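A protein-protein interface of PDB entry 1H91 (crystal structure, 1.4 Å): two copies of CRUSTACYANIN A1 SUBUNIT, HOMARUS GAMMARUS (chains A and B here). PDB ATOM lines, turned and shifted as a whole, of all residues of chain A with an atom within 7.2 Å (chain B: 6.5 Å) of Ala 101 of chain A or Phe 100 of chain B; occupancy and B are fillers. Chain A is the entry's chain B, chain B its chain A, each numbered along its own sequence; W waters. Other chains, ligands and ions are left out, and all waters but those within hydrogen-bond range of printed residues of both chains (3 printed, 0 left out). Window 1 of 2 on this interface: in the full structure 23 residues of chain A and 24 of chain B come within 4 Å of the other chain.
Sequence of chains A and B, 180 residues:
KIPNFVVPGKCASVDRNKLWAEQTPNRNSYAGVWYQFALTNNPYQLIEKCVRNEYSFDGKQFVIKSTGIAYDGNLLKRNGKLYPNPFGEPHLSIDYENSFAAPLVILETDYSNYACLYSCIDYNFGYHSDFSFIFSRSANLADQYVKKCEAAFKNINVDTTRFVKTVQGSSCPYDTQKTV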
ATOM      1  N   TYR A  44      32.118 -10.175  16.960  1.00  0.00           N
ATOM      2  CA  TYR A  44      31.218 -10.242  15.816  1.00  0.00           C
ATOM      3  C   TYR A  44      31.817  -9.670  14.536  1.00  0.00           C
ATOM      4  O   TYR A  44      31.537 -10.152  13.431  1.00  0.00           O
ATOM      5  CB  TYR A  44      29.894  -9.523  16.142  1.00  0.00           C
ATOM      6  CG  TYR A  44      29.265 -10.060  17.414  1.00  0.00           C
ATOM      7  CD1 TYR A  44      29.088  -9.226  18.511  1.00  0.00           C
ATOM      8  CD2 TYR A  44      28.836 -11.389  17.512  1.00  0.00           C
ATOM      9  CE1 TYR A  44      28.505  -9.717  19.670  1.00  0.00           C
ATOM     10  CE2 TYR A  44      28.248 -11.881  18.682  1.00  0.00           C
ATOM     11  CZ  TYR A  44      28.092 -11.029  19.749  1.00  0.00           C
ATOM     12  OH  TYR A  44      27.521 -11.521  20.914  1.00  0.00           O
ATOM     13  N   LYS A  81      22.819  -2.386   6.448  1.00  0.00           N
ATOM     14  CA  LYS A  81      21.793  -1.378   6.481  1.00  0.00           C
ATOM     15  C   LYS A  81      21.712  -0.673   7.837  1.00  0.00           C
ATOM     16  O   LYS A  81      21.984  -1.295   8.864  1.00  0.00           O
ATOM     17  CB  LYS A  81      20.379  -1.904   6.160  1.00  0.00           C
ATOM     18  CG  LYS A  81      20.175  -2.463   4.757  1.00  0.00           C
ATOM     19  CD  LYS A  81      18.839  -3.200   4.670  1.00  0.00           C
ATOM     20  CE  LYS A  81      18.702  -3.883   3.314  1.00  0.00           C
ATOM     21  NZ  LYS A  81      18.278  -2.918   2.268  1.00  0.00           N
ATOM     22  N   TYR A  83      18.824   1.646   9.921  1.00  0.00           N
ATOM     23  CA  TYR A  83      17.428   2.101   9.770  1.00  0.00           C
ATOM     24  C   TYR A  83      16.824   2.385  11.140  1.00  0.00           C
ATOM     25  O   TYR A  83      17.313   1.862  12.143  1.00  0.00           O
ATOM     26  CB  TYR A  83      16.595   1.107   8.966  1.00  0.00           C
ATOM     27  CG  TYR A  83      16.654  -0.356   9.392  1.00  0.00           C
ATOM     28  CD1 TYR A  83      15.930  -0.875  10.463  1.00  0.00           C
ATOM     29  CD2 TYR A  83      17.458  -1.262   8.701  1.00  0.00           C
ATOM     30  CE1 TYR A  83      16.021  -2.225  10.804  1.00  0.00           C
ATOM     31  CE2 TYR A  83      17.569  -2.606   9.014  1.00  0.00           C
ATOM     32  CZ  TYR A  83      16.834  -3.084  10.085  1.00  0.00           C
ATOM     33  OH  TYR A  83      16.926  -4.428  10.431  1.00  0.00           O
ATOM     34  N   PHE A  87      10.409  -0.489  16.699  1.00  0.00           N
ATOM     35  CA  PHE A  87       9.419  -0.208  17.759  1.00  0.00           C
ATOM     36  C   PHE A  87       9.233   1.285  17.997  1.00  0.00           C
ATOM     37  O   PHE A  87       8.445   1.702  18.857  1.00  0.00           O
ATOM     38  CB  PHE A  87       9.866  -0.915  19.061  1.00  0.00           C
ATOM     39  CG  PHE A  87       9.821  -2.435  18.947  1.00  0.00           C
ATOM     40  CD1 PHE A  87      10.961  -3.157  18.601  1.00  0.00           C
ATOM     41  CD2 PHE A  87       8.647  -3.148  19.174  1.00  0.00           C
ATOM     42  CE1 PHE A  87      10.923  -4.529  18.480  1.00  0.00           C
ATOM     43  CE2 PHE A  87       8.631  -4.529  19.065  1.00  0.00           C
ATOM     44  CZ  PHE A  87       9.757  -5.255  18.727  1.00  0.00           C
ATOM     45  N   SER A  93      18.940   0.789  14.195  1.00  0.00           N
ATOM     46  CA  SER A  93      19.339  -0.600  14.086  1.00  0.00           C
ATOM     47  C   SER A  93      20.416  -0.745  13.007  1.00  0.00           C
ATOM     48  O   SER A  93      20.165  -0.305  11.875  1.00  0.00           O
ATOM     49  CB  SER A  93      18.187  -1.523  13.668  1.00  0.00           C
ATOM     50  OG  SER A  93      17.177  -1.562  14.693  1.00  0.00           O
ATOM     51  N   ILE A  94      21.565  -1.301  13.336  1.00  0.00           N
ATOM     52  CA  ILE A  94      22.572  -1.699  12.368  1.00  0.00           C
ATOM     53  C   ILE A  94      22.368  -3.191  12.105  1.00  0.00           C
ATOM     54  O   ILE A  94      22.277  -3.996  13.058  1.00  0.00           O
ATOM     55  CB  ILE A  94      24.015  -1.410  12.802  1.00  0.00           C
ATOM     56  CG1 ILE A  94      25.055  -1.840  11.751  1.00  0.00           C
ATOM     57  CG2 ILE A  94      24.376  -2.034  14.139  1.00  0.00           C
ATOM     58  CD1 ILE A  94      25.099  -0.928  10.543  1.00  0.00           C
ATOM     59  N   ASP A  95      22.224  -3.550  10.841  1.00  0.00           N
ATOM     60  CA  ASP A  95      21.871  -4.882  10.343  1.00  0.00           C
ATOM     61  C   ASP A  95      22.838  -5.307   9.246  1.00  0.00           C
ATOM     62  O   ASP A  95      23.183  -4.502   8.370  1.00  0.00           O
ATOM     63  CB  ASP A  95      20.424  -4.873   9.836  1.00  0.00           C
ATOM     64  CG  ASP A  95      19.771  -6.245   9.809  1.00  0.00           C
ATOM     65  OD1 ASP A  95      18.527  -6.234   9.535  1.00  0.00           O
ATOM     66  OD2 ASP A  95      20.410  -7.284   9.978  1.00  0.00           O
ATOM     67  N   TYR A  96      23.341  -6.546   9.268  1.00  0.00           N
ATOM     68  CA  TYR A  96      24.258  -7.049   8.246  1.00  0.00           C
ATOM     69  C   TYR A  96      23.733  -8.366   7.677  1.00  0.00           C
ATOM     70  O   TYR A  96      23.105  -9.204   8.338  1.00  0.00           O
ATOM     71  CB  TYR A  96      25.699  -7.180   8.777  1.00  0.00           C
ATOM     72  CG  TYR A  96      26.484  -5.880   8.632  1.00  0.00           C
ATOM     73  CD1 TYR A  96      26.379  -4.908   9.613  1.00  0.00           C
ATOM     74  CD2 TYR A  96      27.290  -5.591   7.537  1.00  0.00           C
ATOM     75  CE1 TYR A  96      27.076  -3.707   9.501  1.00  0.00           C
ATOM     76  CE2 TYR A  96      27.990  -4.399   7.412  1.00  0.00           C
ATOM     77  CZ  TYR A  96      27.879  -3.460   8.405  1.00  0.00           C
ATOM     78  OH  TYR A  96      28.574  -2.255   8.283  1.00  0.00           O
ATOM     79  N   SER A  99      23.805 -12.069   9.476  1.00  0.00           N
ATOM     80  CA  SER A  99      24.090 -11.733  10.870  1.00  0.00           C
ATOM     81  C   SER A  99      22.815 -11.325  11.609  1.00  0.00           C
ATOM     82  O   SER A  99      21.696 -11.447  11.132  1.00  0.00           O
ATOM     83  CB  SER A  99      25.130 -10.612  10.900  1.00  0.00           C
ATOM     84  OG  SER A  99      25.273 -10.045  12.189  1.00  0.00           O
ATOM     85  N   PHE A 100      22.968 -10.793  12.795  1.00  0.00           N
ATOM     86  CA  PHE A 100      21.964 -10.179  13.631  1.00  0.00           C
ATOM     87  C   PHE A 100      21.929  -8.664  13.440  1.00  0.00           C
ATOM     88  O   PHE A 100      22.776  -8.059  12.778  1.00  0.00           O
ATOM     89  CB  PHE A 100      22.221 -10.534  15.108  1.00  0.00           C
ATOM     90  CG  PHE A 100      23.628 -10.104  15.475  1.00  0.00           C
ATOM     91  CD1 PHE A 100      23.903  -8.887  16.060  1.00  0.00           C
ATOM     92  CD2 PHE A 100      24.704 -10.946  15.216  1.00  0.00           C
ATOM     93  CE1 PHE A 100      25.197  -8.505  16.355  1.00  0.00           C
ATOM     94  CE2 PHE A 100      26.003 -10.568  15.496  1.00  0.00           C
ATOM     95  CZ  PHE A 100      26.265  -9.339  16.065  1.00  0.00           C
ATOM     96  N   ALA A 101      20.937  -8.028  14.063  1.00  0.00           N
ATOM     97  CA  ALA A 101      20.853  -6.562  14.076  1.00  0.00           C
ATOM     98  C   ALA A 101      20.954  -6.048  15.500  1.00  0.00           C
ATOM     99  O   ALA A 101      20.481  -6.710  16.432  1.00  0.00           O
ATOM    100  CB  ALA A 101      19.568  -6.074  13.431  1.00  0.00           C
ATOM    101  N   ALA A 102      21.570  -4.885  15.705  1.00  0.00           N
ATOM    102  CA  ALA A 102      21.744  -4.411  17.089  1.00  0.00           C
ATOM    103  C   ALA A 102      21.448  -2.924  17.140  1.00  0.00           C
ATOM    104  O   ALA A 102      21.500  -2.269  16.092  1.00  0.00           O
ATOM    105  CB  ALA A 102      23.155  -4.670  17.583  1.00  0.00           C
ATOM    106  N   PRO A 103      21.155  -2.422  18.331  1.00  0.00           N
ATOM    107  CA  PRO A 103      20.974  -0.966  18.417  1.00  0.00           C
ATOM    108  C   PRO A 103      22.317  -0.263  18.188  1.00  0.00           C
ATOM    109  O   PRO A 103      23.372  -0.804  18.563  1.00  0.00           O
ATOM    110  CB  PRO A 103      20.542  -0.739  19.856  1.00  0.00           C
ATOM    111  CG  PRO A 103      20.850  -1.991  20.579  1.00  0.00           C
ATOM    112  CD  PRO A 103      21.009  -3.120  19.616  1.00  0.00           C
ATOM    113  N   SER A 119      26.887   0.606  21.113  1.00  0.00           N
ATOM    114  CA  SER A 119      25.907  -0.456  21.187  1.00  0.00           C
ATOM    115  C   SER A 119      25.946  -1.182  22.538  1.00  0.00           C
ATOM    116  O   SER A 119      27.057  -1.483  23.032  1.00  0.00           O
ATOM    117  CB  SER A 119      26.149  -1.474  20.059  1.00  0.00           C
ATOM    118  OG  SER A 119      25.009  -2.339  19.916  1.00  0.00           O
ATOM    119  N   CYS A 120      24.791  -1.457  23.147  1.00  0.00           N
ATOM    120  CA  CYS A 120      24.747  -2.181  24.425  1.00  0.00           C
ATOM    121  C   CYS A 120      23.544  -3.092  24.477  1.00  0.00           C
ATOM    122  O   CYS A 120      22.484  -2.794  23.916  1.00  0.00           O
ATOM    123  CB  CYS A 120      24.681  -1.183  25.585  1.00  0.00           C
ATOM    124  SG  CYS A 120      24.972  -1.837  27.251  1.00  0.00           S
ATOM    125  N   ILE A 121      23.683  -4.199  25.203  1.00  0.00           N
ATOM    126  CA  ILE A 121      22.611  -5.167  25.385  1.00  0.00           C
ATOM    127  C   ILE A 121      22.585  -5.679  26.820  1.00  0.00           C
ATOM    128  O   ILE A 121      23.662  -6.001  27.349  1.00  0.00           O
ATOM    129  CB  ILE A 121      22.703  -6.392  24.461  1.00  0.00           C
ATOM    130  CG1 ILE A 121      21.506  -7.341  24.649  1.00  0.00           C
ATOM    131  CG2 ILE A 121      24.004  -7.147  24.637  1.00  0.00           C
ATOM    132  CD1 ILE A 121      20.699  -7.624  23.410  1.00  0.00           C
ATOM    133  N   TYR B  44      19.369 -14.074  26.955  1.00  0.00           N
ATOM    134  CA  TYR B  44      18.586 -12.930  26.475  1.00  0.00           C
ATOM    135  C   TYR B  44      17.121 -13.052  26.875  1.00  0.00           C
ATOM    136  O   TYR B  44      16.392 -12.050  26.904  1.00  0.00           O
ATOM    137  CB  TYR B  44      18.661 -12.805  24.960  1.00  0.00           C
ATOM    138  CG  TYR B  44      20.053 -12.761  24.368  1.00  0.00           C
ATOM    139  CD1 TYR B  44      20.540 -13.776  23.561  1.00  0.00           C
ATOM    140  CD2 TYR B  44      20.864 -11.660  24.638  1.00  0.00           C
ATOM    141  CE1 TYR B  44      21.804 -13.776  23.003  1.00  0.00           C
ATOM    142  CE2 TYR B  44      22.141 -11.654  24.071  1.00  0.00           C
ATOM    143  CZ  TYR B  44      22.606 -12.673  23.276  1.00  0.00           C
ATOM    144  OH  TYR B  44      23.880 -12.587  22.754  1.00  0.00           O
ATOM    145  N   TYR B  83       9.403 -10.650  11.367  1.00  0.00           N
ATOM    146  CA  TYR B  83       9.226 -10.153   9.988  1.00  0.00           C
ATOM    147  C   TYR B  83      10.274 -10.713   9.039  1.00  0.00           C
ATOM    148  O   TYR B  83      11.360 -11.130   9.492  1.00  0.00           O
ATOM    149  CB  TYR B  83       9.269  -8.615   9.993  1.00  0.00           C
ATOM    150  CG  TYR B  83      10.385  -7.966  10.791  1.00  0.00           C
ATOM    151  CD1 TYR B  83      11.657  -7.842  10.214  1.00  0.00           C
ATOM    152  CD2 TYR B  83      10.209  -7.466  12.071  1.00  0.00           C
ATOM    153  CE1 TYR B  83      12.686  -7.237  10.943  1.00  0.00           C
ATOM    154  CE2 TYR B  83      11.206  -6.859  12.817  1.00  0.00           C
ATOM    155  CZ  TYR B  83      12.465  -6.762  12.201  1.00  0.00           C
ATOM    156  OH  TYR B  83      13.469  -6.165  12.948  1.00  0.00           O
ATOM    157  N   ILE B  94      13.552 -12.179  14.371  1.00  0.00           N
ATOM    158  CA  ILE B  94      12.814 -12.030  15.650  1.00  0.00           C
ATOM    159  C   ILE B  94      13.397 -10.831  16.413  1.00  0.00           C
ATOM    160  O   ILE B  94      14.609 -10.806  16.699  1.00  0.00           O
ATOM    161  CB  ILE B  94      12.780 -13.285  16.509  1.00  0.00           C
ATOM    162  CG1 ILE B  94      11.941 -13.156  17.804  1.00  0.00           C
ATOM    163  CG2 ILE B  94      14.165 -13.785  16.927  1.00  0.00           C
ATOM    164  CD1 ILE B  94      10.478 -13.499  17.557  1.00  0.00           C
ATOM    165  N   ASP B  95      12.559  -9.801  16.713  1.00  0.00           N
ATOM    166  CA  ASP B  95      12.991  -8.503  17.210  1.00  0.00           C
ATOM    167  C   ASP B  95      12.215  -8.186  18.481  1.00  0.00           C
ATOM    168  O   ASP B  95      10.990  -8.363  18.491  1.00  0.00           O
ATOM    169  CB  ASP B  95      12.801  -7.453  16.104  1.00  0.00           C
ATOM    170  CG  ASP B  95      13.528  -6.143  16.344  1.00  0.00           C
ATOM    171  OD1 ASP B  95      13.559  -5.311  15.396  1.00  0.00           O
ATOM    172  OD2 ASP B  95      14.055  -5.995  17.473  1.00  0.00           O
ATOM    173  N   TYR B  96      12.895  -7.775  19.556  1.00  0.00           N
ATOM    174  CA  TYR B  96      12.176  -7.477  20.800  1.00  0.00           C
ATOM    175  C   TYR B  96      12.486  -6.064  21.272  1.00  0.00           C
ATOM    176  O   TYR B  96      13.595  -5.541  21.042  1.00  0.00           O
ATOM    177  CB  TYR B  96      12.448  -8.542  21.881  1.00  0.00           C
ATOM    178  CG  TYR B  96      11.445  -9.702  21.840  1.00  0.00           C
ATOM    179  CD1 TYR B  96      11.451 -10.678  20.854  1.00  0.00           C
ATOM    180  CD2 TYR B  96      10.457  -9.785  22.805  1.00  0.00           C
ATOM    181  CE1 TYR B  96      10.502 -11.703  20.857  1.00  0.00           C
ATOM    182  CE2 TYR B  96       9.519 -10.795  22.829  1.00  0.00           C
ATOM    183  CZ  TYR B  96       9.551 -11.763  21.846  1.00  0.00           C
ATOM    184  OH  TYR B  96       8.619 -12.790  21.836  1.00  0.00           O
ATOM    185  N   GLU B  97      11.536  -5.389  21.916  1.00  0.00           N
ATOM    186  CA  GLU B  97      11.774  -4.027  22.401  1.00  0.00           C
ATOM    187  C   GLU B  97      12.946  -4.000  23.375  1.00  0.00           C
ATOM    188  O   GLU B  97      13.037  -4.887  24.232  1.00  0.00           O
ATOM    189  CB  GLU B  97      10.504  -3.509  23.077  1.00  0.00           C
ATOM    190  CG  GLU B  97       9.692  -4.624  23.733  1.00  0.00           C
ATOM    191  CD  GLU B  97       8.750  -4.135  24.812  1.00  0.00           C
ATOM    192  OE1 GLU B  97       8.131  -3.074  24.587  1.00  0.00           O
ATOM    193  OE2 GLU B  97       8.640  -4.790  25.870  1.00  0.00           O
ATOM    194  N   ASN B  98      13.831  -3.006  23.273  1.00  0.00           N
ATOM    195  CA  ASN B  98      14.978  -2.876  24.153  1.00  0.00           C
ATOM    196  C   ASN B  98      15.887  -4.102  24.115  1.00  0.00           C
ATOM    197  O   ASN B  98      16.419  -4.510  25.146  1.00  0.00           O
ATOM    198  CB  ASN B  98      14.538  -2.611  25.610  1.00  0.00           C
ATOM    199  CG  ASN B  98      13.999  -1.195  25.705  1.00  0.00           C
ATOM    200  OD1 ASN B  98      12.939  -0.950  26.265  1.00  0.00           O
ATOM    201  ND2 ASN B  98      14.769  -0.283  25.119  1.00  0.00           N
ATOM    202  N   SER B  99      16.076  -4.675  22.936  1.00  0.00           N
ATOM    203  CA  SER B  99      16.920  -5.854  22.737  1.00  0.00           C
ATOM    204  C   SER B  99      17.437  -5.823  21.307  1.00  0.00           C
ATOM    205  O   SER B  99      17.391  -4.832  20.595  1.00  0.00           O
ATOM    206  CB  SER B  99      16.172  -7.158  23.006  1.00  0.00           C
ATOM    207  OG  SER B  99      16.963  -8.332  23.039  1.00  0.00           O
ATOM    208  N   PHE B 100      17.918  -6.943  20.835  1.00  0.00           N
ATOM    209  CA  PHE B 100      18.453  -6.966  19.468  1.00  0.00           C
ATOM    210  C   PHE B 100      17.519  -7.797  18.580  1.00  0.00           C
ATOM    211  O   PHE B 100      16.516  -8.271  19.131  1.00  0.00           O
ATOM    212  CB  PHE B 100      19.853  -7.487  19.586  1.00  0.00           C
ATOM    213  CG  PHE B 100      20.133  -8.970  19.601  1.00  0.00           C
ATOM    214  CD1 PHE B 100      19.881  -9.750  20.713  1.00  0.00           C
ATOM    215  CD2 PHE B 100      20.655  -9.562  18.468  1.00  0.00           C
ATOM    216  CE1 PHE B 100      20.178 -11.108  20.661  1.00  0.00           C
ATOM    217  CE2 PHE B 100      20.963 -10.906  18.414  1.00  0.00           C
ATOM    218  CZ  PHE B 100      20.716 -11.680  19.528  1.00  0.00           C
ATOM    219  N   ALA B 101      17.879  -7.938  17.310  1.00  0.00           N
ATOM    220  CA  ALA B 101      17.111  -8.795  16.399  1.00  0.00           C
ATOM    221  C   ALA B 101      17.986  -9.919  15.861  1.00  0.00           C
ATOM    222  O   ALA B 101      19.160  -9.724  15.616  1.00  0.00           O
ATOM    223  CB  ALA B 101      16.493  -8.012  15.263  1.00  0.00           C
ATOM    224  N   ALA B 102      17.449 -11.113  15.761  1.00  0.00           N
ATOM    225  CA  ALA B 102      18.223 -12.296  15.399  1.00  0.00           C
ATOM    226  C   ALA B 102      17.464 -13.078  14.322  1.00  0.00           C
ATOM    227  O   ALA B 102      16.234 -12.962  14.251  1.00  0.00           O
ATOM    228  CB  ALA B 102      18.491 -13.179  16.612  1.00  0.00           C
ATOM    229  N   PRO B 103      18.204 -13.853  13.544  1.00  0.00           N
ATOM    230  CA  PRO B 103      17.548 -14.762  12.614  1.00  0.00           C
ATOM    231  C   PRO B 103      16.732 -15.821  13.375  1.00  0.00           C
ATOM    232  O   PRO B 103      17.142 -16.288  14.465  1.00  0.00           O
ATOM    233  CB  PRO B 103      18.694 -15.430  11.846  1.00  0.00           C
ATOM    234  CG  PRO B 103      19.857 -15.291  12.804  1.00  0.00           C
ATOM    235  CD  PRO B 103      19.666 -13.975  13.474  1.00  0.00           C
ATOM    236  N   SER B 119      17.944 -20.363  16.168  1.00  0.00           N
ATOM    237  CA  SER B 119      18.651 -19.124  15.836  1.00  0.00           C
ATOM    238  C   SER B 119      20.155 -19.358  15.953  1.00  0.00           C
ATOM    239  O   SER B 119      20.582 -20.099  16.863  1.00  0.00           O
ATOM    240  CB  SER B 119      18.206 -18.006  16.803  1.00  0.00           C
ATOM    241  OG  SER B 119      18.882 -16.773  16.490  1.00  0.00           O
ATOM    242  N   ILE B 121      24.327 -17.501  15.519  1.00  0.00           N
ATOM    243  CA  ILE B 121      25.241 -16.413  15.221  1.00  0.00           C
ATOM    244  C   ILE B 121      26.702 -16.872  15.195  1.00  0.00           C
ATOM    245  O   ILE B 121      27.177 -17.608  16.061  1.00  0.00           O
ATOM    246  CB  ILE B 121      25.165 -15.316  16.320  1.00  0.00           C
ATOM    247  CG1 ILE B 121      23.745 -14.906  16.720  1.00  0.00           C
ATOM    248  CG2 ILE B 121      25.998 -14.117  15.889  1.00  0.00           C
ATOM    249  CD1 ILE B 121      23.102 -15.860  17.710  1.00  0.00           C
ATOM    250  N   PHE B 131      20.722 -21.028  19.705  1.00  0.00           N
ATOM    251  CA  PHE B 131      19.610 -20.843  20.652  1.00  0.00           C
ATOM    252  C   PHE B 131      18.432 -21.580  20.048  1.00  0.00           C
ATOM    253  O   PHE B 131      17.973 -21.217  18.971  1.00  0.00           O
ATOM    254  CB  PHE B 131      19.357 -19.336  20.899  1.00  0.00           C
ATOM    255  CG  PHE B 131      20.621 -18.661  21.451  1.00  0.00           C
ATOM    256  CD1 PHE B 131      21.383 -17.902  20.592  1.00  0.00           C
ATOM    257  CD2 PHE B 131      20.976 -18.851  22.787  1.00  0.00           C
ATOM    258  CE1 PHE B 131      22.567 -17.313  21.031  1.00  0.00           C
ATOM    259  CE2 PHE B 131      22.174 -18.266  23.203  1.00  0.00           C
ATOM    260  CZ  PHE B 131      22.942 -17.505  22.356  1.00  0.00           C
HETATM  261  O   HOH W   1      26.082 -13.625  20.794  1.00  0.00           O
HETATM  262  O   HOH W   2      16.149  -4.173  14.960  1.00  0.00           O
HETATM  263  O   HOH W   3      16.198  -5.853  12.662  1.00  0.00           O
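O of Ala 101 of chain B lies within hydrogen-bond range of N of Ala 101 of chain A (2.9 Å).
Printed residues of chain A that touch a printed residue of chain B: Phe 87, Ser 99, Phe 100, Ala 101 and Ile 121. Hydrophobic or aromatic side chains of chain A that line the printed part of chain B: Phe 87, Phe 100 and Ile 121. Printed residues of chain B that touch a printed residue of chain A: Asp 95, Tyr 96, Glu 97, Ser 99, Phe 100, Ala 101, Pro 103 and Ile 121. Hydrophobic or aromatic side chains of chain B that line the printed part of chain A: Phe 100, Pro 103 and Ile 121.
OH of Tyr 83 of chain B sits at hydrogen-bond distance from OD1 of Asp 95 of chain B (2.6 Å).
Ala 101 of chain A touches just these residues of chain B: Phe 100 and Ala 101. Printed residues of chain A within 4 Å of Phe 100 of chain B: Phe 100, Ala 101 and Ile 121. Of the printed residues of chain B, Ser 99 of chain A touches Pro 103 (3.9996 Å). Printed residues of chain A within 4 Å of Ile 121 of chain B: Phe 100. Of the printed residues of chain A, Glu 97 of chain B touches Phe 87. The nearest residue of chain B that does not touch Ala 101 of chain A is Ala 102 of chain B (5.0 Å). The nearest printed residue of chain A that does not touch Phe 100 of chain B is Ala 102 of chain A (4.4 Å). The nearest printed residue of chain A that does not touch Pro 103 of chain B is Phe 100 of chain A (4.4 Å).
Among the printed residues, pairs that only touch across the chains: Phe 87 of chain A with Asp 95 of chain B, Phe 87 of chain A with Tyr 96 of chain B, Phe 87 of chain A with Glu 97 of chain B, Ser 99 of chain A with Pro 103 of chain B, Phe 100 of chain A with Phe 100 of chain B, Phe 100 of chain A with Ala 101 of chain B, Phe 100 of chain A with Ile 121 of chain B, Ala 101 of chain A with Phe 100 of chain B, Ile 121 of chain A with Ser 99 of chain B and Ile 121 of chain A with Phe 100 of chain B.
Ser 99 of chain A touches Pro 103 of chain B, but with the chains exchanged Pro 103 of chain A does not touch Ser 99 of chain B (4.1 Å). Phe 100 of chain A touches Ala 101 of chain B, and with the chains exchanged Ala 101 of chain A touches Phe 100 of chain B. Phe 100 of chain A touches Ile 121 of chain B, and with the chains exchanged Ile 121 of chain A touches Phe 100 of chain B. Ile 121 of chain A touches Ser 99 of chain B, but with the chains exchanged Ser 99 of chain A does not touch Ile 121 of chain B (5.5 Å).
Water W1 lies within hydrogen-bond range of the side-chain hydroxyl of Tyr 44 of chain A (2.6 Å) and the side-chain hydroxyl of Tyr 44 of chain B (3.1 Å). Water W3 lies within hydrogen-bond range of OH of Tyr 83 of chain A (2.7 Å) and OH of Tyr 83 of chain B (2.8 Å). Water W2 bridges OG of Ser 93 of chain A (2.8 Å) and OD1 of Asp 95 of chain B (2.9 Å).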
